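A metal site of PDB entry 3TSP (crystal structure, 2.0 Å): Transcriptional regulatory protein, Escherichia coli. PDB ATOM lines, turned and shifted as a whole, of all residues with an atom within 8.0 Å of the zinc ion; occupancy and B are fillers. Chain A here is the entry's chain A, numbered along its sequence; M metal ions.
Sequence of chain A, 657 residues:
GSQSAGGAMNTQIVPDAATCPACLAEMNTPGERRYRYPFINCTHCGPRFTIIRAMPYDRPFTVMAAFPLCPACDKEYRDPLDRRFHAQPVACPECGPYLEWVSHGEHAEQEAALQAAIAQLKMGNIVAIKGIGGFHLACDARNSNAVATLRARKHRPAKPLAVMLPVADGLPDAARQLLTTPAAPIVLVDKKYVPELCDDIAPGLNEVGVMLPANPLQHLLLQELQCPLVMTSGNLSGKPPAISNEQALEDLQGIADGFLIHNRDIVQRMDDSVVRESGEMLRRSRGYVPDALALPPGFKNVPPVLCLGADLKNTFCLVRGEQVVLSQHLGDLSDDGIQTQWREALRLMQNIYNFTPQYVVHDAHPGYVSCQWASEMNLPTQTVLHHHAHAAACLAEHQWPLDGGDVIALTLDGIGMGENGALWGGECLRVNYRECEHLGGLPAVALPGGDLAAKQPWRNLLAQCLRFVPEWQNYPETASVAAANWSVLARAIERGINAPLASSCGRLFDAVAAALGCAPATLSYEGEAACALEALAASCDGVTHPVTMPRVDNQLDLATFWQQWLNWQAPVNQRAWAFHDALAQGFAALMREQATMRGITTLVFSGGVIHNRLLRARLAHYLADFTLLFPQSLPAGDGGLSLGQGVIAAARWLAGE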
ATOM      1  N   ALA A  17     -11.670 -12.913 -11.189  1.00  0.00           N
ATOM      2  CA  ALA A  17     -11.254 -12.427  -9.866  1.00  0.00           C
ATOM      3  C   ALA A  17     -12.252 -11.456  -9.253  1.00  0.00           C
ATOM      4  O   ALA A  17     -12.808 -10.616  -9.937  1.00  0.00           O
ATOM      5  CB  ALA A  17      -9.830 -11.808  -9.901  1.00  0.00           C
ATOM      6  N   ALA A  18     -12.452 -11.581  -7.931  1.00  0.00           N
ATOM      7  CA  ALA A  18     -13.347 -10.728  -7.159  1.00  0.00           C
ATOM      8  C   ALA A  18     -12.957  -9.281  -7.315  1.00  0.00           C
ATOM      9  O   ALA A  18     -11.749  -8.965  -7.285  1.00  0.00           O
ATOM     10  CB  ALA A  18     -13.260 -11.125  -5.672  1.00  0.00           C
ATOM     11  N   THR A  19     -13.937  -8.398  -7.483  1.00  0.00           N
ATOM     12  CA  THR A  19     -13.672  -6.946  -7.487  1.00  0.00           C
ATOM     13  C   THR A  19     -12.687  -6.550  -6.350  1.00  0.00           C
ATOM     14  O   THR A  19     -12.911  -6.896  -5.168  1.00  0.00           O
ATOM     15  CB  THR A  19     -15.007  -6.142  -7.384  1.00  0.00           C
ATOM     16  OG1 THR A  19     -15.882  -6.560  -8.449  1.00  0.00           O
ATOM     17  CG2 THR A  19     -14.758  -4.603  -7.498  1.00  0.00           C
ATOM     18  N   CYS A  20     -11.616  -5.821  -6.693  1.00  0.00           N
ATOM     19  CA  CYS A  20     -10.598  -5.465  -5.700  1.00  0.00           C
ATOM     20  C   CYS A  20     -11.040  -4.274  -4.813  1.00  0.00           C
ATOM     21  O   CYS A  20     -12.035  -3.574  -5.114  1.00  0.00           O
ATOM     22  CB  CYS A  20      -9.232  -5.196  -6.374  1.00  0.00           C
ATOM     23  SG  CYS A  20      -9.211  -3.638  -7.331  1.00  0.00           S
ATOM     24  N   PRO A  21     -10.322  -4.056  -3.693  1.00  0.00           N
ATOM     25  CA  PRO A  21     -10.661  -2.890  -2.838  1.00  0.00           C
ATOM     26  C   PRO A  21     -10.576  -1.537  -3.550  1.00  0.00           C
ATOM     27  O   PRO A  21     -11.472  -0.713  -3.398  1.00  0.00           O
ATOM     28  CB  PRO A  21      -9.667  -2.997  -1.672  1.00  0.00           C
ATOM     29  CG  PRO A  21      -9.315  -4.522  -1.645  1.00  0.00           C
ATOM     30  CD  PRO A  21      -9.250  -4.894  -3.103  1.00  0.00           C
ATOM     31  N   ALA A  22      -9.525  -1.311  -4.329  1.00  0.00           N
ATOM     32  CA  ALA A  22      -9.408  -0.091  -5.136  1.00  0.00           C
ATOM     33  C   ALA A  22     -10.574   0.109  -6.119  1.00  0.00           C
ATOM     34  O   ALA A  22     -11.075   1.204  -6.227  1.00  0.00           O
ATOM     35  CB  ALA A  22      -8.035  -0.069  -5.871  1.00  0.00           C
ATOM     36  N   CYS A  23     -11.024  -0.920  -6.839  1.00  0.00           N
ATOM     37  CA  CYS A  23     -12.202  -0.769  -7.700  1.00  0.00           C
ATOM     38  C   CYS A  23     -13.478  -0.532  -6.888  1.00  0.00           C
ATOM     39  O   CYS A  23     -14.367   0.220  -7.301  1.00  0.00           O
ATOM     40  CB  CYS A  23     -12.379  -1.976  -8.630  1.00  0.00           C
ATOM     41  SG  CYS A  23     -11.301  -1.976 -10.065  1.00  0.00           S
ATOM     42  N   LEU A  24     -13.586  -1.184  -5.743  1.00  0.00           N
ATOM     43  CA  LEU A  24     -14.764  -1.007  -4.880  1.00  0.00           C
ATOM     44  C   LEU A  24     -14.822   0.429  -4.348  1.00  0.00           C
ATOM     45  O   LEU A  24     -15.868   1.058  -4.348  1.00  0.00           O
ATOM     46  CB  LEU A  24     -14.769  -2.046  -3.742  1.00  0.00           C
ATOM     47  CG  LEU A  24     -16.026  -2.035  -2.851  1.00  0.00           C
ATOM     48  CD1 LEU A  24     -17.304  -2.211  -3.662  1.00  0.00           C
ATOM     49  CD2 LEU A  24     -15.944  -3.068  -1.760  1.00  0.00           C
ATOM     50  N   GLU A  26     -13.338   3.122  -5.832  1.00  0.00           N
ATOM     51  CA  GLU A  26     -13.659   3.990  -6.979  1.00  0.00           C
ATOM     52  C   GLU A  26     -15.182   4.012  -7.258  1.00  0.00           C
ATOM     53  O   GLU A  26     -15.756   5.079  -7.446  1.00  0.00           O
ATOM     54  CB  GLU A  26     -12.864   3.546  -8.206  1.00  0.00           C
ATOM     55  CG  GLU A  26     -13.057   4.386  -9.462  1.00  0.00           C
ATOM     56  CD  GLU A  26     -12.253   3.878 -10.635  1.00  0.00           C
ATOM     57  OE1 GLU A  26     -11.311   3.033 -10.458  1.00  0.00           O
ATOM     58  OE2 GLU A  26     -12.564   4.305 -11.780  1.00  0.00           O
ATOM     59  N   ILE A  40     -17.185  -2.000 -13.379  1.00  0.00           N
ATOM     60  CA  ILE A  40     -15.846  -1.549 -13.036  1.00  0.00           C
ATOM     61  C   ILE A  40     -14.930  -2.760 -12.801  1.00  0.00           C
ATOM     62  O   ILE A  40     -15.323  -3.767 -12.159  1.00  0.00           O
ATOM     63  CB  ILE A  40     -15.878  -0.621 -11.794  1.00  0.00           C
ATOM     64  CG1 ILE A  40     -14.488  -0.034 -11.516  1.00  0.00           C
ATOM     65  CG2 ILE A  40     -16.441  -1.353 -10.545  1.00  0.00           C
ATOM     66  CD1 ILE A  40     -14.551   1.172 -10.542  1.00  0.00           C
ATOM     67  N   ASN A  41     -13.734  -2.673 -13.392  1.00  0.00           N
ATOM     68  CA  ASN A  41     -12.659  -3.677 -13.167  1.00  0.00           C
ATOM     69  C   ASN A  41     -11.328  -3.006 -13.428  1.00  0.00           C
ATOM     70  O   ASN A  41     -11.292  -1.888 -13.939  1.00  0.00           O
ATOM     71  CB  ASN A  41     -12.824  -4.937 -14.052  1.00  0.00           C
ATOM     72  CG  ASN A  41     -12.980  -4.622 -15.532  1.00  0.00           C
ATOM     73  OD1 ASN A  41     -14.087  -4.671 -16.067  1.00  0.00           O
ATOM     74  ND2 ASN A  41     -11.879  -4.310 -16.226  1.00  0.00           N
ATOM     75  N   CYS A  42     -10.256  -3.659 -13.055  1.00  0.00           N
ATOM     76  CA  CYS A  42      -8.927  -3.146 -13.362  1.00  0.00           C
ATOM     77  C   CYS A  42      -7.995  -4.297 -13.711  1.00  0.00           C
ATOM     78  O   CYS A  42      -8.420  -5.420 -13.910  1.00  0.00           O
ATOM     79  CB  CYS A  42      -8.379  -2.325 -12.183  1.00  0.00           C
ATOM     80  SG  CYS A  42      -7.889  -3.317 -10.758  1.00  0.00           S
ATOM     81  N   THR A  43      -6.708  -4.011 -13.781  1.00  0.00           N
ATOM     82  CA  THR A  43      -5.764  -5.039 -14.159  1.00  0.00           C
ATOM     83  C   THR A  43      -5.689  -6.169 -13.123  1.00  0.00           C
ATOM     84  O   THR A  43      -5.312  -7.298 -13.461  1.00  0.00           O
ATOM     85  CB  THR A  43      -4.376  -4.440 -14.521  1.00  0.00           C
ATOM     86  OG1 THR A  43      -3.637  -5.410 -15.264  1.00  0.00           O
ATOM     87  CG2 THR A  43      -3.580  -4.008 -13.259  1.00  0.00           C
ATOM     88  N   HIS A  44      -6.111  -5.883 -11.893  1.00  0.00           N
ATOM     89  CA  HIS A  44      -6.115  -6.850 -10.781  1.00  0.00           C
ATOM     90  C   HIS A  44      -7.407  -7.628 -10.555  1.00  0.00           C
ATOM     91  O   HIS A  44      -7.409  -8.592  -9.785  1.00  0.00           O
ATOM     92  CB  HIS A  44      -5.676  -6.171  -9.487  1.00  0.00           C
ATOM     93  CG  HIS A  44      -4.332  -5.509  -9.610  1.00  0.00           C
ATOM     94  ND1 HIS A  44      -4.170  -4.144  -9.557  1.00  0.00           N
ATOM     95  CD2 HIS A  44      -3.104  -6.037  -9.839  1.00  0.00           C
ATOM     96  CE1 HIS A  44      -2.887  -3.862  -9.717  1.00  0.00           C
ATOM     97  NE2 HIS A  44      -2.219  -4.992  -9.899  1.00  0.00           N
ATOM     98  N   CYS A  45      -8.510  -7.230 -11.174  1.00  0.00           N
ATOM     99  CA  CYS A  45      -9.764  -7.881 -10.864  1.00  0.00           C
ATOM    100  C   CYS A  45     -10.686  -7.930 -12.065  1.00  0.00           C
ATOM    101  O   CYS A  45     -10.408  -7.321 -13.102  1.00  0.00           O
ATOM    102  CB  CYS A  45     -10.465  -7.201  -9.675  1.00  0.00           C
ATOM    103  SG  CYS A  45     -11.214  -5.654 -10.059  1.00  0.00           S
ATOM    104  N   GLY A  46     -11.799  -8.657 -11.918  1.00  0.00           N
ATOM    105  CA  GLY A  46     -12.772  -8.658 -12.962  1.00  0.00           C
ATOM    106  C   GLY A  46     -12.799 -10.005 -13.668  1.00  0.00           C
ATOM    107  O   GLY A  46     -12.037 -10.906 -13.336  1.00  0.00           O
ATOM    108  N   ARG A  48     -12.296 -12.905 -16.409  1.00  0.00           N
ATOM    109  CA  ARG A  48     -11.159 -13.304 -17.254  1.00  0.00           C
ATOM    110  C   ARG A  48     -11.609 -14.417 -18.214  1.00  0.00           C
ATOM    111  O   ARG A  48     -12.101 -14.138 -19.322  1.00  0.00           O
ATOM    112  CB  ARG A  48      -9.987 -13.758 -16.355  1.00  0.00           C
ATOM    113  CG  ARG A  48      -9.402 -12.654 -15.500  1.00  0.00           C
ATOM    114  CD  ARG A  48      -8.616 -11.640 -16.348  1.00  0.00           C
ATOM    115  NE  ARG A  48      -8.003 -10.593 -15.528  1.00  0.00           N
ATOM    116  CZ  ARG A  48      -8.590  -9.451 -15.187  1.00  0.00           C
ATOM    117  NH1 ARG A  48      -7.937  -8.579 -14.430  1.00  0.00           N
ATOM    118  NH2 ARG A  48      -9.856  -9.174 -15.570  1.00  0.00           N
ATOM    119  N   ARG A  83      -3.689   1.843 -12.790  1.00  0.00           N
ATOM    120  CA  ARG A  83      -4.177   0.543 -12.325  1.00  0.00           C
ATOM    121  C   ARG A  83      -4.983  -0.213 -13.397  1.00  0.00           C
ATOM    122  O   ARG A  83      -5.132  -1.436 -13.311  1.00  0.00           O
ATOM    123  CB  ARG A  83      -5.019   0.692 -11.045  1.00  0.00           C
ATOM    124  CG  ARG A  83      -5.252  -0.665 -10.346  1.00  0.00           C
ATOM    125  CD  ARG A  83      -6.066  -0.555  -9.078  1.00  0.00           C
ATOM    126  NE  ARG A  83      -7.484  -0.421  -9.344  1.00  0.00           N
ATOM    127  CZ  ARG A  83      -8.167   0.729  -9.321  1.00  0.00           C
ATOM    128  NH1 ARG A  83      -7.574   1.873  -9.055  1.00  0.00           N
ATOM    129  NH2 ARG A  83      -9.468   0.714  -9.556  1.00  0.00           N
ATOM    130  N   ARG A  84      -5.469   0.521 -14.400  1.00  0.00           N
ATOM    131  CA  ARG A  84      -6.245  -0.072 -15.488  1.00  0.00           C
ATOM    132  C   ARG A  84      -5.424  -0.282 -16.772  1.00  0.00           C
ATOM    133  O   ARG A  84      -5.989  -0.569 -17.839  1.00  0.00           O
ATOM    134  CB  ARG A  84      -7.503   0.749 -15.768  1.00  0.00           C
ATOM    135  CG  ARG A  84      -8.454   0.721 -14.586  1.00  0.00           C
ATOM    136  CD  ARG A  84      -9.345   1.925 -14.566  1.00  0.00           C
ATOM    137  NE  ARG A  84      -9.418   2.556 -13.235  1.00  0.00           N
ATOM    138  CZ  ARG A  84      -8.721   3.645 -12.860  1.00  0.00           C
ATOM    139  NH1 ARG A  84      -7.868   4.249 -13.688  1.00  0.00           N
ATOM    140  NH2 ARG A  84      -8.891   4.129 -11.629  1.00  0.00           N
ATOM    141  N   ALA A  87      -6.197  -3.226 -18.845  1.00  0.00           N
ATOM    142  CA  ALA A  87      -7.336  -3.942 -18.257  1.00  0.00           C
ATOM    143  C   ALA A  87      -8.263  -4.253 -19.448  1.00  0.00           C
ATOM    144  O   ALA A  87      -8.985  -3.360 -19.939  1.00  0.00           O
ATOM    145  CB  ALA A  87      -8.033  -3.103 -17.197  1.00  0.00           C
HETATM  146 ZN    ZN M   1      -9.904  -3.790  -9.582  1.00  0.00          ZN
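The guanidinium group (NH1) of Arg 48 is in hydrogen-bond range of the backbone carbonyl oxygen (O) of Cys 45 (3.1 Å).
SG of Cys 23 sits close to NH2 of Arg 83 (3.3 Å).
The side-chain sulfur of Cys 42 lies close to the guanidinium group of Arg 83.
SG of Cys 42 lies close to N of His 44, 3.3 Å away.
The backbone carbonyl oxygen (O) of Cys 42 is in hydrogen-bond range of the guanidinium group (NH1) of Arg 48, at 3.2 Å.
Of the 20 residues printed, 4 come within 4 Å of the zinc ion.
The nearest printed residue that does not touch the zinc ion is Arg 83 (4.2 Å).
The zinc ion is bound by the side-chain sulfur of Cys 45 (2.3 Å), the side-chain sulfur of Cys 23 (2.3 Å), the side-chain sulfur of Cys 20 (2.4 Å) and the side-chain sulfur of Cys 42 (2.4 Å).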
